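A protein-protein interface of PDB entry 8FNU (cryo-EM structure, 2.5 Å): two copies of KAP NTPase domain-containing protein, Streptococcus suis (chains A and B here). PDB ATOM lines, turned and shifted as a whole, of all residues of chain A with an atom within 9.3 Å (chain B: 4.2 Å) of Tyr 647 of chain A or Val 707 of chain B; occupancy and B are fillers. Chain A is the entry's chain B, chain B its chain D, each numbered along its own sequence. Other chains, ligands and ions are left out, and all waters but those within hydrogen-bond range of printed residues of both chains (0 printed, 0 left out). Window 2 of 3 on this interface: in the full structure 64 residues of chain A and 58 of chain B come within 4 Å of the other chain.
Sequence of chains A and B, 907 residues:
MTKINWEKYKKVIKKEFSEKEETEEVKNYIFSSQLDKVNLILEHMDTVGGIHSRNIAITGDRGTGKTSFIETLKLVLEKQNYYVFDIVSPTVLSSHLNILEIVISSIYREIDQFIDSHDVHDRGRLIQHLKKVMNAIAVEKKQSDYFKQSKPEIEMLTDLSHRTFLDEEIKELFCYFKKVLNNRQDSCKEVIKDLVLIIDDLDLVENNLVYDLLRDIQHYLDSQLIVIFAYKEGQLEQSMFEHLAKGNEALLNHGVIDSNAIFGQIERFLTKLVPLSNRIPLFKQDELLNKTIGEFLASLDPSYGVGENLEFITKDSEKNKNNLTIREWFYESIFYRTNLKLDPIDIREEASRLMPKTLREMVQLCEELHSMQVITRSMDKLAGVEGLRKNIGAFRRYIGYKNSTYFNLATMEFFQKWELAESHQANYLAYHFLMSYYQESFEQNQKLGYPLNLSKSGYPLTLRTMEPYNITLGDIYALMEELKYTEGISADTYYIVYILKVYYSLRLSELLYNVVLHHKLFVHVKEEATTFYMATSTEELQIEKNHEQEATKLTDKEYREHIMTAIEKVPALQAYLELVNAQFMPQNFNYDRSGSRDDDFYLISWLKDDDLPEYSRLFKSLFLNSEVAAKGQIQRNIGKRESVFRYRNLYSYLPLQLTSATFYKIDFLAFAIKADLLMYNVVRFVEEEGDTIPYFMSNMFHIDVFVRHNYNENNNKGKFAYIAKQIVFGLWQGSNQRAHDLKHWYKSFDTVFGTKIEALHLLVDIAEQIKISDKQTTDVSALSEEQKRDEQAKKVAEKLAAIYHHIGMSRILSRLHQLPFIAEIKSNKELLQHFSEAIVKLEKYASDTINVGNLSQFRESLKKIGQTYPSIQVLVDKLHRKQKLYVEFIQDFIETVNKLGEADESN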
ATOM      1  N   THR A 465     -32.175 -17.733 -23.819  1.00  0.00           N
ATOM      2  CA  THR A 465     -31.318 -18.904 -23.634  1.00  0.00           C
ATOM      3  C   THR A 465     -30.055 -18.742 -24.482  1.00  0.00           C
ATOM      4  O   THR A 465     -29.683 -19.581 -25.305  1.00  0.00           O
ATOM      5  CB  THR A 465     -32.072 -20.181 -23.979  1.00  0.00           C
ATOM      6  OG1 THR A 465     -32.435 -20.168 -25.364  1.00  0.00           O
ATOM      7  CG2 THR A 465     -33.332 -20.289 -23.132  1.00  0.00           C
ATOM      8  N   MET A 466     -29.392 -17.614 -24.240  1.00  0.00           N
ATOM      9  CA  MET A 466     -28.260 -17.137 -25.017  1.00  0.00           C
ATOM     10  C   MET A 466     -27.116 -16.867 -24.052  1.00  0.00           C
ATOM     11  O   MET A 466     -27.336 -16.489 -22.897  1.00  0.00           O
ATOM     12  CB  MET A 466     -28.616 -15.840 -25.773  1.00  0.00           C
ATOM     13  CG  MET A 466     -27.854 -15.386 -27.060  1.00  0.00           C
ATOM     14  SD  MET A 466     -27.372 -16.361 -28.538  1.00  0.00           S
ATOM     15  CE  MET A 466     -27.572 -18.108 -28.219  1.00  0.00           C
ATOM     16  N   GLU A 467     -25.894 -17.075 -24.523  1.00  0.00           N
ATOM     17  CA  GLU A 467     -24.737 -16.859 -23.669  1.00  0.00           C
ATOM     18  C   GLU A 467     -24.596 -15.368 -23.366  1.00  0.00           C
ATOM     19  O   GLU A 467     -25.022 -14.527 -24.162  1.00  0.00           O
ATOM     20  CB  GLU A 467     -23.473 -17.352 -24.359  1.00  0.00           C
ATOM     21  CG  GLU A 467     -23.390 -18.842 -24.666  1.00  0.00           C
ATOM     22  CD  GLU A 467     -24.555 -19.707 -24.250  1.00  0.00           C
ATOM     23  OE1 GLU A 467     -24.293 -20.905 -24.044  1.00  0.00           O
ATOM     24  OE2 GLU A 467     -25.711 -19.246 -24.168  1.00  0.00           O
ATOM     25  N   PRO A 468     -24.005 -15.005 -22.225  1.00  0.00           N
ATOM     26  CA  PRO A 468     -23.667 -13.588 -22.015  1.00  0.00           C
ATOM     27  C   PRO A 468     -22.687 -13.050 -23.040  1.00  0.00           C
ATOM     28  O   PRO A 468     -22.708 -11.846 -23.325  1.00  0.00           O
ATOM     29  CB  PRO A 468     -23.072 -13.562 -20.600  1.00  0.00           C
ATOM     30  CG  PRO A 468     -23.507 -14.815 -19.962  1.00  0.00           C
ATOM     31  CD  PRO A 468     -23.699 -15.827 -21.042  1.00  0.00           C
ATOM     32  N   TYR A 469     -21.830 -13.899 -23.607  1.00  0.00           N
ATOM     33  CA  TYR A 469     -20.900 -13.492 -24.650  1.00  0.00           C
ATOM     34  C   TYR A 469     -21.509 -13.564 -26.041  1.00  0.00           C
ATOM     35  O   TYR A 469     -20.784 -13.425 -27.031  1.00  0.00           O
ATOM     36  CB  TYR A 469     -19.620 -14.340 -24.597  1.00  0.00           C
ATOM     37  CG  TYR A 469     -19.821 -15.828 -24.455  1.00  0.00           C
ATOM     38  CD1 TYR A 469     -20.011 -16.631 -25.564  1.00  0.00           C
ATOM     39  CD2 TYR A 469     -19.778 -16.435 -23.208  1.00  0.00           C
ATOM     40  CE1 TYR A 469     -20.178 -17.989 -25.439  1.00  0.00           C
ATOM     41  CE2 TYR A 469     -19.943 -17.795 -23.073  1.00  0.00           C
ATOM     42  CZ  TYR A 469     -20.136 -18.568 -24.193  1.00  0.00           C
ATOM     43  OH  TYR A 469     -20.306 -19.928 -24.070  1.00  0.00           O
ATOM     44  N   ASN A 470     -22.823 -13.773 -26.140  1.00  0.00           N
ATOM     45  CA  ASN A 470     -23.523 -13.774 -27.417  1.00  0.00           C
ATOM     46  C   ASN A 470     -24.620 -12.715 -27.465  1.00  0.00           C
ATOM     47  O   ASN A 470     -25.552 -12.829 -28.269  1.00  0.00           O
ATOM     48  CB  ASN A 470     -24.102 -15.160 -27.699  1.00  0.00           C
ATOM     49  CG  ASN A 470     -23.030 -16.184 -28.010  1.00  0.00           C
ATOM     50  OD1 ASN A 470     -21.978 -15.850 -28.551  1.00  0.00           O
ATOM     51  ND2 ASN A 470     -23.293 -17.439 -27.677  1.00  0.00           N
ATOM     52  N   PHE A 645     -21.970 -26.573 -30.363  1.00  0.00           N
ATOM     53  CA  PHE A 645     -22.686 -25.413 -30.880  1.00  0.00           C
ATOM     54  C   PHE A 645     -23.401 -24.671 -29.750  1.00  0.00           C
ATOM     55  O   PHE A 645     -24.377 -23.961 -29.990  1.00  0.00           O
ATOM     56  CB  PHE A 645     -23.696 -25.838 -31.949  1.00  0.00           C
ATOM     57  CG  PHE A 645     -24.695 -26.853 -31.468  1.00  0.00           C
ATOM     58  CD1 PHE A 645     -25.900 -26.450 -30.919  1.00  0.00           C
ATOM     59  CD2 PHE A 645     -24.432 -28.209 -31.570  1.00  0.00           C
ATOM     60  CE1 PHE A 645     -26.822 -27.378 -30.476  1.00  0.00           C
ATOM     61  CE2 PHE A 645     -25.352 -29.141 -31.130  1.00  0.00           C
ATOM     62  CZ  PHE A 645     -26.548 -28.724 -30.581  1.00  0.00           C
ATOM     63  N   ARG A 646     -22.909 -24.839 -28.519  1.00  0.00           N
ATOM     64  CA  ARG A 646     -23.578 -24.305 -27.339  1.00  0.00           C
ATOM     65  C   ARG A 646     -22.774 -23.276 -26.559  1.00  0.00           C
ATOM     66  O   ARG A 646     -23.375 -22.377 -25.963  1.00  0.00           O
ATOM     67  CB  ARG A 646     -23.946 -25.439 -26.374  1.00  0.00           C
ATOM     68  CG  ARG A 646     -25.431 -25.667 -26.255  1.00  0.00           C
ATOM     69  CD  ARG A 646     -25.759 -26.795 -25.298  1.00  0.00           C
ATOM     70  NE  ARG A 646     -26.948 -26.472 -24.519  1.00  0.00           N
ATOM     71  CZ  ARG A 646     -27.485 -27.259 -23.598  1.00  0.00           C
ATOM     72  NH1 ARG A 646     -26.962 -28.436 -23.300  1.00  0.00           N
ATOM     73  NH2 ARG A 646     -28.579 -26.853 -22.959  1.00  0.00           N
ATOM     74  N   TYR A 647     -21.451 -23.379 -26.545  1.00  0.00           N
ATOM     75  CA  TYR A 647     -20.594 -22.592 -25.663  1.00  0.00           C
ATOM     76  C   TYR A 647     -19.679 -21.703 -26.477  1.00  0.00           C
ATOM     77  O   TYR A 647     -18.467 -21.643 -26.255  1.00  0.00           O
ATOM     78  CB  TYR A 647     -19.786 -23.500 -24.745  1.00  0.00           C
ATOM     79  CG  TYR A 647     -20.644 -24.470 -23.979  1.00  0.00           C
ATOM     80  CD1 TYR A 647     -21.463 -24.027 -22.954  1.00  0.00           C
ATOM     81  CD2 TYR A 647     -20.642 -25.822 -24.280  1.00  0.00           C
ATOM     82  CE1 TYR A 647     -22.253 -24.902 -22.246  1.00  0.00           C
ATOM     83  CE2 TYR A 647     -21.429 -26.708 -23.578  1.00  0.00           C
ATOM     84  CZ  TYR A 647     -22.234 -26.242 -22.560  1.00  0.00           C
ATOM     85  OH  TYR A 647     -23.024 -27.117 -21.853  1.00  0.00           O
ATOM     86  N   ARG A 648     -20.262 -20.999 -27.435  1.00  0.00           N
ATOM     87  CA  ARG A 648     -19.512 -20.434 -28.539  1.00  0.00           C
ATOM     88  C   ARG A 648     -19.604 -18.916 -28.589  1.00  0.00           C
ATOM     89  O   ARG A 648     -20.686 -18.335 -28.474  1.00  0.00           O
ATOM     90  CB  ARG A 648     -20.015 -21.073 -29.826  1.00  0.00           C
ATOM     91  CG  ARG A 648     -19.514 -22.504 -29.911  1.00  0.00           C
ATOM     92  CD  ARG A 648     -19.073 -22.823 -31.294  1.00  0.00           C
ATOM     93  NE  ARG A 648     -18.249 -23.955 -31.621  1.00  0.00           N
ATOM     94  CZ  ARG A 648     -17.758 -24.173 -32.831  1.00  0.00           C
ATOM     95  NH1 ARG A 648     -18.552 -24.260 -33.884  1.00  0.00           N
ATOM     96  NH2 ARG A 648     -16.444 -24.288 -32.992  1.00  0.00           N
ATOM     97  N   ASN A 649     -18.441 -18.286 -28.767  1.00  0.00           N
ATOM     98  CA  ASN A 649     -18.342 -16.836 -28.658  1.00  0.00           C
ATOM     99  C   ASN A 649     -19.123 -16.150 -29.770  1.00  0.00           C
ATOM    100  O   ASN A 649     -19.773 -15.123 -29.542  1.00  0.00           O
ATOM    101  CB  ASN A 649     -16.869 -16.428 -28.679  1.00  0.00           C
ATOM    102  CG  ASN A 649     -16.263 -16.379 -27.291  1.00  0.00           C
ATOM    103  OD1 ASN A 649     -16.180 -15.320 -26.669  1.00  0.00           O
ATOM    104  ND2 ASN A 649     -15.846 -17.539 -26.790  1.00  0.00           N
ATOM    105  N   LEU A 650     -19.040 -16.690 -30.984  1.00  0.00           N
ATOM    106  CA  LEU A 650     -19.835 -16.277 -32.136  1.00  0.00           C
ATOM    107  C   LEU A 650     -19.470 -14.881 -32.630  1.00  0.00           C
ATOM    108  O   LEU A 650     -19.921 -14.471 -33.704  1.00  0.00           O
ATOM    109  CB  LEU A 650     -21.335 -16.282 -31.808  1.00  0.00           C
ATOM    110  CG  LEU A 650     -22.183 -17.552 -32.003  1.00  0.00           C
ATOM    111  CD1 LEU A 650     -23.555 -17.496 -31.312  1.00  0.00           C
ATOM    112  CD2 LEU A 650     -22.255 -18.119 -33.414  1.00  0.00           C
ATOM    113  N   TYR B 477     -26.273 -32.884 -13.620  1.00  0.00           N
ATOM    114  CA  TYR B 477     -25.654 -31.832 -14.416  1.00  0.00           C
ATOM    115  C   TYR B 477     -26.459 -31.544 -15.676  1.00  0.00           C
ATOM    116  O   TYR B 477     -26.586 -30.385 -16.085  1.00  0.00           O
ATOM    117  CB  TYR B 477     -24.223 -32.222 -14.779  1.00  0.00           C
ATOM    118  CG  TYR B 477     -23.500 -31.137 -15.531  1.00  0.00           C
ATOM    119  CD1 TYR B 477     -22.834 -30.127 -14.856  1.00  0.00           C
ATOM    120  CD2 TYR B 477     -23.507 -31.106 -16.917  1.00  0.00           C
ATOM    121  CE1 TYR B 477     -22.184 -29.129 -15.538  1.00  0.00           C
ATOM    122  CE2 TYR B 477     -22.860 -30.109 -17.608  1.00  0.00           C
ATOM    123  CZ  TYR B 477     -22.199 -29.124 -16.915  1.00  0.00           C
ATOM    124  OH  TYR B 477     -21.554 -28.127 -17.606  1.00  0.00           O
ATOM    125  N   GLU B 481     -28.039 -27.956 -16.648  1.00  0.00           N
ATOM    126  CA  GLU B 481     -27.810 -27.277 -17.921  1.00  0.00           C
ATOM    127  C   GLU B 481     -29.124 -26.963 -18.631  1.00  0.00           C
ATOM    128  O   GLU B 481     -29.322 -25.843 -19.116  1.00  0.00           O
ATOM    129  CB  GLU B 481     -26.909 -28.126 -18.819  1.00  0.00           C
ATOM    130  CG  GLU B 481     -25.440 -28.148 -18.422  1.00  0.00           C
ATOM    131  CD  GLU B 481     -24.886 -26.773 -18.095  1.00  0.00           C
ATOM    132  OE1 GLU B 481     -24.589 -26.010 -19.038  1.00  0.00           O
ATOM    133  OE2 GLU B 481     -24.747 -26.457 -16.895  1.00  0.00           O
ATOM    134  N   TYR B 485     -30.800 -23.389 -19.737  1.00  0.00           N
ATOM    135  CA  TYR B 485     -31.187 -23.056 -21.104  1.00  0.00           C
ATOM    136  C   TYR B 485     -32.696 -23.161 -21.313  1.00  0.00           C
ATOM    137  O   TYR B 485     -33.152 -23.468 -22.415  1.00  0.00           O
ATOM    138  CB  TYR B 485     -30.455 -23.961 -22.090  1.00  0.00           C
ATOM    139  CG  TYR B 485     -28.999 -23.624 -22.227  1.00  0.00           C
ATOM    140  CD1 TYR B 485     -28.071 -24.092 -21.310  1.00  0.00           C
ATOM    141  CD2 TYR B 485     -28.553 -22.828 -23.262  1.00  0.00           C
ATOM    142  CE1 TYR B 485     -26.739 -23.783 -21.428  1.00  0.00           C
ATOM    143  CE2 TYR B 485     -27.229 -22.515 -23.388  1.00  0.00           C
ATOM    144  CZ  TYR B 485     -26.320 -22.993 -22.469  1.00  0.00           C
ATOM    145  OH  TYR B 485     -24.988 -22.679 -22.591  1.00  0.00           O
ATOM    146  N   PHE B 589     -24.882 -36.931 -24.256  1.00  0.00           N
ATOM    147  CA  PHE B 589     -23.879 -35.983 -24.710  1.00  0.00           C
ATOM    148  C   PHE B 589     -23.363 -36.345 -26.096  1.00  0.00           C
ATOM    149  O   PHE B 589     -23.142 -37.517 -26.413  1.00  0.00           O
ATOM    150  CB  PHE B 589     -22.724 -35.929 -23.711  1.00  0.00           C
ATOM    151  CG  PHE B 589     -21.708 -34.868 -24.014  1.00  0.00           C
ATOM    152  CD1 PHE B 589     -22.026 -33.529 -23.867  1.00  0.00           C
ATOM    153  CD2 PHE B 589     -20.436 -35.206 -24.434  1.00  0.00           C
ATOM    154  CE1 PHE B 589     -21.097 -32.552 -24.142  1.00  0.00           C
ATOM    155  CE2 PHE B 589     -19.502 -34.231 -24.710  1.00  0.00           C
ATOM    156  CZ  PHE B 589     -19.833 -32.902 -24.563  1.00  0.00           C
ATOM    157  N   ILE B 703     -16.943 -31.017 -15.007  1.00  0.00           N
ATOM    158  CA  ILE B 703     -17.956 -31.375 -15.999  1.00  0.00           C
ATOM    159  C   ILE B 703     -18.276 -30.172 -16.878  1.00  0.00           C
ATOM    160  O   ILE B 703     -18.541 -30.313 -18.080  1.00  0.00           O
ATOM    161  CB  ILE B 703     -19.223 -31.926 -15.316  1.00  0.00           C
ATOM    162  CG1 ILE B 703     -18.879 -33.058 -14.344  1.00  0.00           C
ATOM    163  CG2 ILE B 703     -20.202 -32.436 -16.360  1.00  0.00           C
ATOM    164  CD1 ILE B 703     -20.000 -33.391 -13.383  1.00  0.00           C
ATOM    165  N   ASP B 704     -18.278 -28.974 -16.288  1.00  0.00           N
ATOM    166  CA  ASP B 704     -18.404 -27.760 -17.088  1.00  0.00           C
ATOM    167  C   ASP B 704     -17.343 -27.720 -18.173  1.00  0.00           C
ATOM    168  O   ASP B 704     -17.643 -27.451 -19.340  1.00  0.00           O
ATOM    169  CB  ASP B 704     -18.293 -26.521 -16.196  1.00  0.00           C
ATOM    170  CG  ASP B 704     -19.639 -25.986 -15.759  1.00  0.00           C
ATOM    171  OD1 ASP B 704     -20.630 -26.738 -15.815  1.00  0.00           O
ATOM    172  OD2 ASP B 704     -19.705 -24.806 -15.357  1.00  0.00           O
ATOM    173  N   VAL B 705     -16.092 -27.997 -17.808  1.00  0.00           N
ATOM    174  CA  VAL B 705     -15.025 -28.004 -18.802  1.00  0.00           C
ATOM    175  C   VAL B 705     -15.234 -29.133 -19.807  1.00  0.00           C
ATOM    176  O   VAL B 705     -15.008 -28.963 -21.011  1.00  0.00           O
ATOM    177  CB  VAL B 705     -13.658 -28.112 -18.106  1.00  0.00           C
ATOM    178  CG1 VAL B 705     -12.549 -28.237 -19.133  1.00  0.00           C
ATOM    179  CG2 VAL B 705     -13.426 -26.914 -17.214  1.00  0.00           C
ATOM    180  N   PHE B 706     -15.664 -30.303 -19.328  1.00  0.00           N
ATOM    181  CA  PHE B 706     -15.796 -31.467 -20.197  1.00  0.00           C
ATOM    182  C   PHE B 706     -16.822 -31.228 -21.294  1.00  0.00           C
ATOM    183  O   PHE B 706     -16.584 -31.560 -22.460  1.00  0.00           O
ATOM    184  CB  PHE B 706     -16.185 -32.694 -19.370  1.00  0.00           C
ATOM    185  CG  PHE B 706     -15.063 -33.264 -18.546  1.00  0.00           C
ATOM    186  CD1 PHE B 706     -13.784 -33.373 -19.061  1.00  0.00           C
ATOM    187  CD2 PHE B 706     -15.294 -33.695 -17.251  1.00  0.00           C
ATOM    188  CE1 PHE B 706     -12.760 -33.896 -18.299  1.00  0.00           C
ATOM    189  CE2 PHE B 706     -14.274 -34.217 -16.488  1.00  0.00           C
ATOM    190  CZ  PHE B 706     -13.006 -34.319 -17.012  1.00  0.00           C
ATOM    191  N   VAL B 707     -17.978 -30.660 -20.942  1.00  0.00           N
ATOM    192  CA  VAL B 707     -18.997 -30.404 -21.954  1.00  0.00           C
ATOM    193  C   VAL B 707     -18.533 -29.355 -22.955  1.00  0.00           C
ATOM    194  O   VAL B 707     -19.061 -29.292 -24.071  1.00  0.00           O
ATOM    195  CB  VAL B 707     -20.331 -29.984 -21.308  1.00  0.00           C
ATOM    196  CG1 VAL B 707     -20.868 -31.102 -20.429  1.00  0.00           C
ATOM    197  CG2 VAL B 707     -20.178 -28.696 -20.514  1.00  0.00           C
ATOM    198  N   ARG B 708     -17.556 -28.525 -22.586  1.00  0.00           N
ATOM    199  CA  ARG B 708     -17.016 -27.520 -23.492  1.00  0.00           C
ATOM    200  C   ARG B 708     -15.948 -28.071 -24.428  1.00  0.00           C
ATOM    201  O   ARG B 708     -15.616 -27.408 -25.417  1.00  0.00           O
ATOM    202  CB  ARG B 708     -16.418 -26.360 -22.691  1.00  0.00           C
ATOM    203  CG  ARG B 708     -17.310 -25.138 -22.580  1.00  0.00           C
ATOM    204  CD  ARG B 708     -18.318 -25.286 -21.464  1.00  0.00           C
ATOM    205  NE  ARG B 708     -18.878 -24.007 -21.047  1.00  0.00           N
ATOM    206  CZ  ARG B 708     -19.823 -23.872 -20.125  1.00  0.00           C
ATOM    207  NH1 ARG B 708     -20.326 -24.918 -19.493  1.00  0.00           N
ATOM    208  NH2 ARG B 708     -20.276 -22.656 -19.835  1.00  0.00           N
ATOM    209  N   HIS B 709     -15.408 -29.253 -24.147  1.00  0.00           N
ATOM    210  CA  HIS B 709     -14.303 -29.785 -24.927  1.00  0.00           C
ATOM    211  C   HIS B 709     -14.766 -30.165 -26.333  1.00  0.00           C
ATOM    212  O   HIS B 709     -15.943 -30.446 -26.580  1.00  0.00           O
ATOM    213  CB  HIS B 709     -13.694 -30.994 -24.218  1.00  0.00           C
ATOM    214  CG  HIS B 709     -12.343 -31.381 -24.730  1.00  0.00           C
ATOM    215  ND1 HIS B 709     -11.201 -30.672 -24.426  1.00  0.00           N
ATOM    216  CD2 HIS B 709     -11.947 -32.413 -25.512  1.00  0.00           C
ATOM    217  CE1 HIS B 709     -10.162 -31.244 -25.007  1.00  0.00           C
ATOM    218  NE2 HIS B 709     -10.587 -32.303 -25.671  1.00  0.00           N
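No position is printed for both chains.
Of the 7 pairs that touch across the chains among the printed residues, none has its exchanged pair printed and touching as well.
Printed residues of chain B within 4 Å of Thr 465 of chain A: Tyr 485 (3.3 Å).
Of the printed residues of chain B, Glu 467 of chain A touches Tyr 485.
Of the printed residues of chain B, Arg 646 of chain A touches Tyr 485 (3.3 Å).
Of chain B, only Glu 481 (3.4 Å), Tyr 485 (3.5 Å), Val 707 (3.5 Å) and Arg 708 (3.2 Å) come within 4 Å of Tyr 647 of chain A.
Arg 648 of chain A touches none of the printed residues of chain B.
Of the printed residues of chain A, Glu 481 of chain B touches Tyr 647 (3.4 Å).
Of the printed residues of chain A, Tyr 485 of chain B touches Thr 465, Glu 467, Arg 646 and Tyr 647.
Phe 589 of chain B touches none of the printed residues of chain A.
Arg 708 of chain B touches just one residue of chain A: Tyr 647.
The nearest residue of chain A that does not touch Val 707 of chain B is Arg 646 of chain A (6.6 Å).
The nearest printed residue of chain B that does not touch Arg 646 of chain A is Glu 481 of chain B (4.04 Å).
Of the 12 printed residues of chain A, 4 touch a printed residue of chain B.
Printed residues of chain A that touch a printed residue of chain B: Thr 465, Glu 467, Arg 646 and Tyr 647.
Hydrophobic or aromatic side chains of chain A that line the printed part of chain B: Tyr 647.
Hydrophobic or aromatic side chains of chain B that line the printed part of chain A: Tyr 485 and Val 707.
Among the printed residues, 7 pairs touch across the chains.
OH of Tyr 647 of chain A is in hydrogen-bond range of OE1 of Glu 481 of chain B, at 3.4 Å.
OE1 of Glu 467 of chain A lies close to OH of Tyr 485 of chain B, 2.4 Å away.
OE1 of Glu 467 of chain A sits close to O of Arg 646 of chain A (2.6 Å).
The side-chain hydroxyl of Tyr 469 of chain A sits close to the backbone carbonyl oxygen of Tyr 647 of chain A, 3.3 Å away.
Among the printed residues, merely in contact across the chains: Thr 465 of chain A with Tyr 485 of chain B (3.3 Å), Arg 646 of chain A with Tyr 485 of chain B (3.3 Å), Tyr 647 of chain A with Tyr 485 of chain B (3.5 Å), Tyr 647 of chain A with Val 707 of chain B (3.5 Å) and Tyr 647 of chain A with Arg 708 of chain B (3.2 Å).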
